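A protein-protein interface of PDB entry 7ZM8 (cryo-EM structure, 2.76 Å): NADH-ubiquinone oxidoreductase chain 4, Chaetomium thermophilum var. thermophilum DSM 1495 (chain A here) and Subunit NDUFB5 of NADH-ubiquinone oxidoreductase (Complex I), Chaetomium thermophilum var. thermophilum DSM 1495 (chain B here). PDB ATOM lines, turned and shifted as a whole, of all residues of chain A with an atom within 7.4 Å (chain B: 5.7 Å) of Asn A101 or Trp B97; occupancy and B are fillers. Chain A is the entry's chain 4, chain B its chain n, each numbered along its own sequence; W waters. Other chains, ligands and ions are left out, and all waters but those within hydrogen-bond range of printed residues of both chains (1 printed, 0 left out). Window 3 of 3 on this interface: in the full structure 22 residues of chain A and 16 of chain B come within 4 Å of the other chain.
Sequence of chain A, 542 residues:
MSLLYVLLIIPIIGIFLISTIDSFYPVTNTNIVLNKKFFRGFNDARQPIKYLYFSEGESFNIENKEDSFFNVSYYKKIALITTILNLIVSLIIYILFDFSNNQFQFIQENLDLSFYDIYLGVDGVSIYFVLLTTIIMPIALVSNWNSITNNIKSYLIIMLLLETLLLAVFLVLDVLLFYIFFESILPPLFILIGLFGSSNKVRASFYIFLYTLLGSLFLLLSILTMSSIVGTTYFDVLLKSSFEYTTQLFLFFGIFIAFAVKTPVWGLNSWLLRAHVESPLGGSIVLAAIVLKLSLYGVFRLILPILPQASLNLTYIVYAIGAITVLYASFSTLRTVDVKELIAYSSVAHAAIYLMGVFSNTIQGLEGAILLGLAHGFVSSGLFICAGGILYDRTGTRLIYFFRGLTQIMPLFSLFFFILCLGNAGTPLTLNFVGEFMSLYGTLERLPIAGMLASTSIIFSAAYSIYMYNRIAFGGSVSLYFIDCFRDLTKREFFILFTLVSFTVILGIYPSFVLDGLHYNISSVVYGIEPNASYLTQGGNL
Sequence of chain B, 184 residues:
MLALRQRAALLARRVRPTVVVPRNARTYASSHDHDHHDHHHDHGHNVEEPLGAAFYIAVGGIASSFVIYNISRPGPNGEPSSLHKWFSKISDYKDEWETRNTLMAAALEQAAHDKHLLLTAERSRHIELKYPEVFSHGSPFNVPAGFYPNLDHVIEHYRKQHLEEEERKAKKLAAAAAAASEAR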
ATOM      1  N   SER A   2      13.432  11.419  -0.677  1.00  0.00           N
ATOM      2  CA  SER A   2      12.467  10.375  -0.376  1.00  0.00           C
ATOM      3  C   SER A   2      12.456   9.316  -1.471  1.00  0.00           C
ATOM      4  O   SER A   2      13.120   9.438  -2.502  1.00  0.00           O
ATOM      5  CB  SER A   2      11.066  10.957  -0.218  1.00  0.00           C
ATOM      6  OG  SER A   2      10.092   9.931  -0.257  1.00  0.00           O
ATOM      7  N   LEU A  96       7.386  -2.251   1.965  1.00  0.00           N
ATOM      8  CA  LEU A  96       7.562  -1.497   3.197  1.00  0.00           C
ATOM      9  C   LEU A  96       6.269  -0.884   3.708  1.00  0.00           C
ATOM     10  O   LEU A  96       6.221  -0.467   4.867  1.00  0.00           O
ATOM     11  CB  LEU A  96       8.603  -0.399   2.978  1.00  0.00           C
ATOM     12  CG  LEU A  96       9.903  -0.879   2.334  1.00  0.00           C
ATOM     13  CD1 LEU A  96      10.787   0.286   1.934  1.00  0.00           C
ATOM     14  CD2 LEU A  96      10.636  -1.814   3.268  1.00  0.00           C
ATOM     15  N   PHE A  97       5.231  -0.843   2.883  1.00  0.00           N
ATOM     16  CA  PHE A  97       4.031  -0.080   3.187  1.00  0.00           C
ATOM     17  C   PHE A  97       3.277  -0.669   4.374  1.00  0.00           C
ATOM     18  O   PHE A  97       3.170  -1.888   4.516  1.00  0.00           O
ATOM     19  CB  PHE A  97       3.137  -0.045   1.950  1.00  0.00           C
ATOM     20  CG  PHE A  97       1.930   0.819   2.094  1.00  0.00           C
ATOM     21  CD1 PHE A  97       2.043   2.190   2.046  1.00  0.00           C
ATOM     22  CD2 PHE A  97       0.680   0.261   2.261  1.00  0.00           C
ATOM     23  CE1 PHE A  97       0.939   2.984   2.171  1.00  0.00           C
ATOM     24  CE2 PHE A  97      -0.419   1.053   2.387  1.00  0.00           C
ATOM     25  CZ  PHE A  97      -0.288   2.418   2.344  1.00  0.00           C
ATOM     26  N   ASP A  98       2.778   0.205   5.263  1.00  0.00           N
ATOM     27  CA  ASP A  98       1.973  -0.236   6.438  1.00  0.00           C
ATOM     28  C   ASP A  98       0.504  -0.257   6.050  1.00  0.00           C
ATOM     29  O   ASP A  98      -0.032   0.814   5.794  1.00  0.00           O
ATOM     30  CB  ASP A  98       2.133   0.708   7.626  1.00  0.00           C
ATOM     31  CG  ASP A  98       1.642   0.139   8.946  1.00  0.00           C
ATOM     32  OD1 ASP A  98       0.420   0.082   9.144  1.00  0.00           O
ATOM     33  OD2 ASP A  98       2.494  -0.243   9.766  1.00  0.00           O
ATOM     34  N   PHE A  99      -0.125  -1.425   6.051  1.00  0.00           N
ATOM     35  CA  PHE A  99      -1.523  -1.577   5.577  1.00  0.00           C
ATOM     36  C   PHE A  99      -2.534  -1.023   6.574  1.00  0.00           C
ATOM     37  O   PHE A  99      -3.688  -0.912   6.180  1.00  0.00           O
ATOM     38  CB  PHE A  99      -1.877  -3.041   5.328  1.00  0.00           C
ATOM     39  CG  PHE A  99      -1.245  -3.709   4.139  1.00  0.00           C
ATOM     40  CD1 PHE A  99      -0.733  -2.970   3.087  1.00  0.00           C
ATOM     41  CD2 PHE A  99      -1.203  -5.089   4.062  1.00  0.00           C
ATOM     42  CE1 PHE A  99      -0.171  -3.603   1.993  1.00  0.00           C
ATOM     43  CE2 PHE A  99      -0.638  -5.720   2.967  1.00  0.00           C
ATOM     44  CZ  PHE A  99      -0.123  -4.974   1.937  1.00  0.00           C
ATOM     45  N   SER A 100      -2.160  -0.735   7.818  1.00  0.00           N
ATOM     46  CA  SER A 100      -3.156  -0.110   8.724  1.00  0.00           C
ATOM     47  C   SER A 100      -2.589   1.132   9.406  1.00  0.00           C
ATOM     48  O   SER A 100      -2.539   1.140  10.631  1.00  0.00           O
ATOM     49  CB  SER A 100      -3.674  -1.092   9.718  1.00  0.00           C
ATOM     50  OG  SER A 100      -2.627  -1.621  10.516  1.00  0.00           O
ATOM     51  N   ASN A 101      -2.266   2.170   8.637  1.00  0.00           N
ATOM     52  CA  ASN A 101      -1.678   3.418   9.183  1.00  0.00           C
ATOM     53  C   ASN A 101      -2.481   4.616   8.680  1.00  0.00           C
ATOM     54  O   ASN A 101      -2.772   4.654   7.492  1.00  0.00           O
ATOM     55  CB  ASN A 101      -0.196   3.527   8.827  1.00  0.00           C
ATOM     56  CG  ASN A 101       0.578   4.524   9.660  1.00  0.00           C
ATOM     57  OD1 ASN A 101       0.049   5.118  10.594  1.00  0.00           O
ATOM     58  ND2 ASN A 101       1.846   4.705   9.335  1.00  0.00           N
ATOM     59  N   ASN A 102      -2.832   5.551   9.556  1.00  0.00           N
ATOM     60  CA  ASN A 102      -3.670   6.710   9.158  1.00  0.00           C
ATOM     61  C   ASN A 102      -2.796   7.919   8.841  1.00  0.00           C
ATOM     62  O   ASN A 102      -3.353   8.964   8.503  1.00  0.00           O
ATOM     63  CB  ASN A 102      -4.801   7.005  10.145  1.00  0.00           C
ATOM     64  CG  ASN A 102      -4.400   7.772  11.383  1.00  0.00           C
ATOM     65  OD1 ASN A 102      -3.252   7.740  11.819  1.00  0.00           O
ATOM     66  ND2 ASN A 102      -5.367   8.454  11.968  1.00  0.00           N
ATOM     67  N   GLN A 103      -1.483   7.784   8.951  1.00  0.00           N
ATOM     68  CA  GLN A 103      -0.563   8.882   8.574  1.00  0.00           C
ATOM     69  C   GLN A 103      -0.056   8.647   7.153  1.00  0.00           C
ATOM     70  O   GLN A 103       0.215   7.491   6.847  1.00  0.00           O
ATOM     71  CB  GLN A 103       0.630   8.926   9.534  1.00  0.00           C
ATOM     72  CG  GLN A 103       0.261   9.149  10.990  1.00  0.00           C
ATOM     73  CD  GLN A 103      -0.070  10.590  11.283  1.00  0.00           C
ATOM     74  OE1 GLN A 103       0.102  11.466  10.446  1.00  0.00           O
ATOM     75  NE2 GLN A 103      -0.548  10.847  12.487  1.00  0.00           N
ATOM     76  N   PHE A 104       0.109   9.689   6.333  1.00  0.00           N
ATOM     77  CA  PHE A 104       0.737   9.509   4.993  1.00  0.00           C
ATOM     78  C   PHE A 104       2.170   9.000   5.170  1.00  0.00           C
ATOM     79  O   PHE A 104       2.869   9.480   6.059  1.00  0.00           O
ATOM     80  CB  PHE A 104       0.644  10.757   4.114  1.00  0.00           C
ATOM     81  CG  PHE A 104      -0.726  11.092   3.591  1.00  0.00           C
ATOM     82  CD1 PHE A 104      -1.261  10.403   2.516  1.00  0.00           C
ATOM     83  CD2 PHE A 104      -1.461  12.123   4.152  1.00  0.00           C
ATOM     84  CE1 PHE A 104      -2.515  10.726   2.027  1.00  0.00           C
ATOM     85  CE2 PHE A 104      -2.716  12.443   3.663  1.00  0.00           C
ATOM     86  CZ  PHE A 104      -3.240  11.742   2.602  1.00  0.00           C
ATOM     87  N   GLN A 105       2.591   8.047   4.335  1.00  0.00           N
ATOM     88  CA  GLN A 105       3.916   7.395   4.480  1.00  0.00           C
ATOM     89  C   GLN A 105       4.911   7.823   3.394  1.00  0.00           C
ATOM     90  O   GLN A 105       4.449   8.332   2.376  1.00  0.00           O
ATOM     91  CB  GLN A 105       3.699   5.885   4.508  1.00  0.00           C
ATOM     92  CG  GLN A 105       2.602   5.440   5.458  1.00  0.00           C
ATOM     93  CD  GLN A 105       2.292   3.977   5.291  1.00  0.00           C
ATOM     94  OE1 GLN A 105       3.155   3.182   4.945  1.00  0.00           O
ATOM     95  NE2 GLN A 105       1.048   3.609   5.530  1.00  0.00           N
ATOM     96  N   PHE A 106       6.216   7.596   3.600  1.00  0.00           N
ATOM     97  CA  PHE A 106       7.296   7.931   2.673  1.00  0.00           C
ATOM     98  C   PHE A 106       7.281   9.407   2.300  1.00  0.00           C
ATOM     99  O   PHE A 106       7.607   9.784   1.176  1.00  0.00           O
ATOM    100  CB  PHE A 106       7.254   7.034   1.437  1.00  0.00           C
ATOM    101  CG  PHE A 106       7.301   5.573   1.767  1.00  0.00           C
ATOM    102  CD1 PHE A 106       8.504   4.937   1.967  1.00  0.00           C
ATOM    103  CD2 PHE A 106       6.135   4.846   1.907  1.00  0.00           C
ATOM    104  CE1 PHE A 106       8.543   3.601   2.281  1.00  0.00           C
ATOM    105  CE2 PHE A 106       6.168   3.510   2.224  1.00  0.00           C
ATOM    106  CZ  PHE A 106       7.369   2.886   2.408  1.00  0.00           C
ATOM    107  N   ILE A 107       6.915  10.246   3.262  1.00  0.00           N
ATOM    108  CA  ILE A 107       6.892  11.689   3.082  1.00  0.00           C
ATOM    109  C   ILE A 107       8.282  12.234   3.363  1.00  0.00           C
ATOM    110  O   ILE A 107       9.134  11.537   3.923  1.00  0.00           O
ATOM    111  CB  ILE A 107       5.864  12.358   4.007  1.00  0.00           C
ATOM    112  CG1 ILE A 107       6.250  12.111   5.456  1.00  0.00           C
ATOM    113  CG2 ILE A 107       4.491  11.800   3.763  1.00  0.00           C
ATOM    114  CD1 ILE A 107       5.452  12.914   6.420  1.00  0.00           C
ATOM    115  N   GLN A 108       8.518  13.484   2.983  1.00  0.00           N
ATOM    116  CA  GLN A 108       9.777  14.159   3.256  1.00  0.00           C
ATOM    117  C   GLN A 108       9.491  15.453   4.000  1.00  0.00           C
ATOM    118  O   GLN A 108       8.553  16.179   3.653  1.00  0.00           O
ATOM    119  CB  GLN A 108      10.542  14.443   1.963  1.00  0.00           C
ATOM    120  CG  GLN A 108      12.024  14.691   2.175  1.00  0.00           C
ATOM    121  CD  GLN A 108      12.761  14.931   0.876  1.00  0.00           C
ATOM    122  OE1 GLN A 108      12.147  15.094  -0.178  1.00  0.00           O
ATOM    123  NE2 GLN A 108      14.087  14.954   0.943  1.00  0.00           N
ATOM    124  N   VAL A 122       1.983   8.543   0.498  1.00  0.00           N
ATOM    125  CA  VAL A 122       1.244   7.377   0.037  1.00  0.00           C
ATOM    126  C   VAL A 122       0.332   6.881   1.152  1.00  0.00           C
ATOM    127  O   VAL A 122       0.718   6.855   2.326  1.00  0.00           O
ATOM    128  CB  VAL A 122       2.194   6.261  -0.466  1.00  0.00           C
ATOM    129  CG1 VAL A 122       2.929   5.588   0.680  1.00  0.00           C
ATOM    130  CG2 VAL A 122       1.437   5.244  -1.297  1.00  0.00           C
ATOM    131  N   ASP A 123      -0.892   6.517   0.746  1.00  0.00           N
ATOM    132  CA  ASP A 123      -1.871   5.889   1.668  1.00  0.00           C
ATOM    133  C   ASP A 123      -2.403   4.670   0.918  1.00  0.00           C
ATOM    134  O   ASP A 123      -2.153   4.580  -0.288  1.00  0.00           O
ATOM    135  CB  ASP A 123      -3.029   6.821   2.008  1.00  0.00           C
ATOM    136  CG  ASP A 123      -3.008   7.280   3.452  1.00  0.00           C
ATOM    137  OD1 ASP A 123      -1.906   7.440   3.997  1.00  0.00           O
ATOM    138  OD2 ASP A 123      -4.094   7.464   4.021  1.00  0.00           O
ATOM    139  N   GLY A 124      -3.072   3.754   1.607  1.00  0.00           N
ATOM    140  CA  GLY A 124      -3.606   2.559   0.983  1.00  0.00           C
ATOM    141  C   GLY A 124      -4.566   2.872  -0.140  1.00  0.00           C
ATOM    142  O   GLY A 124      -4.751   2.064  -1.050  1.00  0.00           O
ATOM    143  N   GLY A 517      -4.982  -3.976   1.854  1.00  0.00           N
ATOM    144  CA  GLY A 517      -4.295  -2.684   1.933  1.00  0.00           C
ATOM    145  C   GLY A 517      -5.308  -1.579   2.057  1.00  0.00           C
ATOM    146  O   GLY A 517      -4.984  -0.582   2.696  1.00  0.00           O
ATOM    147  N   TYR A 520      -8.437  -0.259   6.087  1.00  0.00           N
ATOM    148  CA  TYR A 520      -8.308   0.807   7.108  1.00  0.00           C
ATOM    149  C   TYR A 520      -8.450   2.194   6.473  1.00  0.00           C
ATOM    150  O   TYR A 520      -9.081   3.070   7.066  1.00  0.00           O
ATOM    151  CB  TYR A 520      -6.968   0.596   7.808  1.00  0.00           C
ATOM    152  CG  TYR A 520      -6.663   1.569   8.910  1.00  0.00           C
ATOM    153  CD1 TYR A 520      -7.108   1.341  10.198  1.00  0.00           C
ATOM    154  CD2 TYR A 520      -5.928   2.709   8.659  1.00  0.00           C
ATOM    155  CE1 TYR A 520      -6.841   2.232  11.219  1.00  0.00           C
ATOM    156  CE2 TYR A 520      -5.654   3.611   9.667  1.00  0.00           C
ATOM    157  CZ  TYR A 520      -6.111   3.372  10.946  1.00  0.00           C
ATOM    158  OH  TYR A 520      -5.834   4.265  11.930  1.00  0.00           O
ATOM    159  N   ASN A 521      -7.812   2.407   5.333  1.00  0.00           N
ATOM    160  CA  ASN A 521      -7.848   3.711   4.620  1.00  0.00           C
ATOM    161  C   ASN A 521      -9.230   3.976   4.010  1.00  0.00           C
ATOM    162  O   ASN A 521      -9.605   5.141   3.920  1.00  0.00           O
ATOM    163  CB  ASN A 521      -6.628   3.878   3.708  1.00  0.00           C
ATOM    164  CG  ASN A 521      -5.316   3.837   4.468  1.00  0.00           C
ATOM    165  OD1 ASN A 521      -4.361   3.208   4.032  1.00  0.00           O
ATOM    166  ND2 ASN A 521      -5.252   4.484   5.617  1.00  0.00           N
ATOM    167  N   TYR B  93       9.601   2.171  11.362  1.00  0.00           N
ATOM    168  CA  TYR B  93       8.991   3.497  11.290  1.00  0.00           C
ATOM    169  C   TYR B  93       8.010   3.719  12.439  1.00  0.00           C
ATOM    170  O   TYR B  93       6.870   4.152  12.246  1.00  0.00           O
ATOM    171  CB  TYR B  93       8.305   3.705   9.943  1.00  0.00           C
ATOM    172  CG  TYR B  93       9.186   3.409   8.758  1.00  0.00           C
ATOM    173  CD1 TYR B  93      10.478   3.888   8.701  1.00  0.00           C
ATOM    174  CD2 TYR B  93       8.718   2.661   7.693  1.00  0.00           C
ATOM    175  CE1 TYR B  93      11.286   3.631   7.625  1.00  0.00           C
ATOM    176  CE2 TYR B  93       9.517   2.394   6.609  1.00  0.00           C
ATOM    177  CZ  TYR B  93      10.803   2.882   6.579  1.00  0.00           C
ATOM    178  OH  TYR B  93      11.610   2.622   5.497  1.00  0.00           O
ATOM    179  N   ASP B  95       7.364   5.782  14.812  1.00  0.00           N
ATOM    180  CA  ASP B  95       6.591   7.016  14.868  1.00  0.00           C
ATOM    181  C   ASP B  95       7.107   8.082  13.910  1.00  0.00           C
ATOM    182  O   ASP B  95       6.669   9.234  13.993  1.00  0.00           O
ATOM    183  CB  ASP B  95       6.585   7.580  16.292  1.00  0.00           C
ATOM    184  CG  ASP B  95       7.973   7.634  16.902  1.00  0.00           C
ATOM    185  OD1 ASP B  95       8.932   7.164  16.253  1.00  0.00           O
ATOM    186  OD2 ASP B  95       8.109   8.151  18.030  1.00  0.00           O
ATOM    187  N   GLU B  96       8.014   7.739  12.996  1.00  0.00           N
ATOM    188  CA  GLU B  96       8.680   8.784  12.230  1.00  0.00           C
ATOM    189  C   GLU B  96       7.816   9.284  11.079  1.00  0.00           C
ATOM    190  O   GLU B  96       8.093  10.353  10.527  1.00  0.00           O
ATOM    191  CB  GLU B  96      10.051   8.303  11.750  1.00  0.00           C
ATOM    192  CG  GLU B  96      10.051   7.117  10.828  1.00  0.00           C
ATOM    193  CD  GLU B  96       9.874   7.523   9.387  1.00  0.00           C
ATOM    194  OE1 GLU B  96      10.127   8.704   9.065  1.00  0.00           O
ATOM    195  OE2 GLU B  96       9.473   6.669   8.578  1.00  0.00           O
ATOM    196  N   TRP B  97       6.776   8.543  10.691  1.00  0.00           N
ATOM    197  CA  TRP B  97       5.776   9.140   9.811  1.00  0.00           C
ATOM    198  C   TRP B  97       4.911  10.135  10.571  1.00  0.00           C
ATOM    199  O   TRP B  97       4.578  11.203  10.049  1.00  0.00           O
ATOM    200  CB  TRP B  97       4.888   8.080   9.151  1.00  0.00           C
ATOM    201  CG  TRP B  97       5.577   7.051   8.300  1.00  0.00           C
ATOM    202  CD1 TRP B  97       5.278   5.725   8.238  1.00  0.00           C
ATOM    203  CD2 TRP B  97       6.656   7.260   7.380  1.00  0.00           C
ATOM    204  NE1 TRP B  97       6.105   5.094   7.349  1.00  0.00           N
ATOM    205  CE2 TRP B  97       6.961   6.014   6.808  1.00  0.00           C
ATOM    206  CE3 TRP B  97       7.398   8.379   6.989  1.00  0.00           C
ATOM    207  CZ2 TRP B  97       7.974   5.852   5.874  1.00  0.00           C
ATOM    208  CZ3 TRP B  97       8.403   8.215   6.064  1.00  0.00           C
ATOM    209  CH2 TRP B  97       8.689   6.960   5.523  1.00  0.00           C
ATOM    210  N   GLU B  98       4.540   9.802  11.807  1.00  0.00           N
ATOM    211  CA  GLU B  98       3.719  10.709  12.600  1.00  0.00           C
ATOM    212  C   GLU B  98       4.456  11.998  12.938  1.00  0.00           C
ATOM    213  O   GLU B  98       3.870  13.084  12.864  1.00  0.00           O
ATOM    214  CB  GLU B  98       3.247  10.016  13.873  1.00  0.00           C
ATOM    215  CG  GLU B  98       2.221  10.826  14.617  1.00  0.00           C
ATOM    216  CD  GLU B  98       2.872  11.870  15.506  1.00  0.00           C
ATOM    217  OE1 GLU B  98       4.007  11.634  15.971  1.00  0.00           O
ATOM    218  OE2 GLU B  98       2.295  12.962  15.664  1.00  0.00           O
ATOM    219  N   THR B  99       5.724  11.904  13.332  1.00  0.00           N
ATOM    220  CA  THR B  99       6.428  13.107  13.758  1.00  0.00           C
ATOM    221  C   THR B  99       6.663  14.055  12.593  1.00  0.00           C
ATOM    222  O   THR B  99       6.702  15.272  12.786  1.00  0.00           O
ATOM    223  CB  THR B  99       7.751  12.741  14.435  1.00  0.00           C
ATOM    224  OG1 THR B  99       8.393  13.932  14.908  1.00  0.00           O
ATOM    225  CG2 THR B  99       8.678  12.038  13.473  1.00  0.00           C
ATOM    226  N   ARG B 100       6.709  13.541  11.377  1.00  0.00           N
ATOM    227  CA  ARG B 100       7.036  14.419  10.231  1.00  0.00           C
ATOM    228  C   ARG B 100       5.743  14.988   9.676  1.00  0.00           C
ATOM    229  O   ARG B 100       5.759  16.137   9.243  1.00  0.00           O
ATOM    230  CB  ARG B 100       7.804  13.618   9.180  1.00  0.00           C
ATOM    231  CG  ARG B 100       9.229  13.265   9.574  1.00  0.00           C
ATOM    232  CD  ARG B 100       9.855  12.371   8.525  1.00  0.00           C
ATOM    233  NE  ARG B 100      11.172  11.900   8.923  1.00  0.00           N
ATOM    234  CZ  ARG B 100      12.308  12.530   8.656  1.00  0.00           C
ATOM    235  NH1 ARG B 100      12.290  13.667   7.981  1.00  0.00           N
ATOM    236  NH2 ARG B 100      13.458  12.023   9.061  1.00  0.00           N
ATOM    237  N   ASN B 101       4.676  14.208   9.709  1.00  0.00           N
ATOM    238  CA  ASN B 101       3.346  14.663   9.237  1.00  0.00           C
ATOM    239  C   ASN B 101       2.829  15.752  10.148  1.00  0.00           C
ATOM    240  O   ASN B 101       2.243  16.699   9.638  1.00  0.00           O
ATOM    241  CB  ASN B 101       2.327  13.523   9.204  1.00  0.00           C
ATOM    242  CG  ASN B 101       2.382  12.695   7.939  1.00  0.00           C
ATOM    243  OD1 ASN B 101       2.095  13.185   6.854  1.00  0.00           O
ATOM    244  ND2 ASN B 101       2.731  11.431   8.069  1.00  0.00           N
ATOM    245  N   THR B 102       3.011  15.581  11.450  1.00  0.00           N
ATOM    246  CA  THR B 102       2.512  16.556  12.447  1.00  0.00           C
ATOM    247  C   THR B 102       3.224  17.892  12.290  1.00  0.00           C
ATOM    248  O   THR B 102       2.546  18.920  12.362  1.00  0.00           O
ATOM    249  CB  THR B 102       2.598  15.963  13.855  1.00  0.00           C
ATOM    250  OG1 THR B 102       1.982  14.682  13.763  1.00  0.00           O
ATOM    251  CG2 THR B 102       1.889  16.798  14.896  1.00  0.00           C
HETATM  252  O   HOH W   1      -0.947  12.283   7.913  1.00  0.00           O
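The side-chain amide nitrogen (ND2) of Asn B101 lies within hydrogen-bond range of the backbone carbonyl oxygen (O) of Phe A104, at 2.8 Å.
The backbone carbonyl oxygen (O) of Asn A101 sits at hydrogen-bond distance from the side-chain amide nitrogen (ND2) of Asn A521 (3.1 Å).
OD1 of Asp A98 sits at hydrogen-bond distance from N of Asn A101 (3.4 Å).
The backbone carbonyl oxygen of Phe A106 is in hydrogen-bond range of the side-chain hydroxyl of Ser A2 (2.9 Å).
The side-chain carboxylate (OE1) of Glu B96 is in salt-bridge range of the guanidinium group (NE) of Arg B100.
N of Gln A105 sits at hydrogen-bond distance from O of Val A122 (3.0 Å).
O of Asp A98 lies within hydrogen-bond range of NE2 of Gln A105 (3.0 Å).
Asn A101 touches Trp B97 (ND2 to CD1, 3.7 Å).
Glu B98 touches Gln A103.
Gln A103 touches Asn B101 (OE1 to CB, 3.3 Å).
CB of Trp B97 touches O of Phe A104, at 3.9 Å.
NE1 of Trp B97 touches CB of Gln A105 (3.8 Å).
Phe A106 touches Trp B97.
N of Ile A107 touches CZ3 of Trp B97, 3.8 Å away.
Ile A107 touches Arg B100.
CD1 of Ile A107 touches OD1 of Asn B101 (3.4 Å).
Asn A101 touches one residue of chain B.
Trp B97 touches just these residues of chain A: Asn A101 (3.7 Å), Phe A104 (3.9 Å), Gln A105 (3.8 Å), Phe A106 (3.2 Å) and Ile A107 (3.8 Å).
Printed residues of chain B within 4 Å of Phe A106: Trp B97.
Printed residues of chain A within 4 Å of Asn B101: Gln A103, Phe A104 and Ile A107.
Of the printed residues of chain B, Gln A105 touches Trp B97 (3.8 Å).
Of the printed residues of chain B, Gln A103 touches Glu B98 and Asn B101.
Of the printed residues of chain A, Arg B100 touches Ile A107 (3.7 Å).
The nearest printed residue of chain B that does not touch Phe A106 is Tyr B93 (4.6 Å).
Of the 20 printed residues of chain A, 6 touch a printed residue of chain B.
Printed residues of chain A that touch a printed residue of chain B: Asn A101, Gln A103, Phe A104, Gln A105, Phe A106 and Ile A107.
Of the 9 printed residues of chain B, 4 touch a printed residue of chain A.
Printed residues of chain B that touch a printed residue of chain A: Trp B97, Glu B98, Arg B100 and Asn B101.
Among the printed residues, no Asp or Glu carboxylate lies within 4 Å of a Lys or Arg side-chain nitrogen of the other chain.
Water W1 lies within hydrogen-bond range of OE1 of Gln A103, N of Phe A104 and OD1 of Asn B101.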
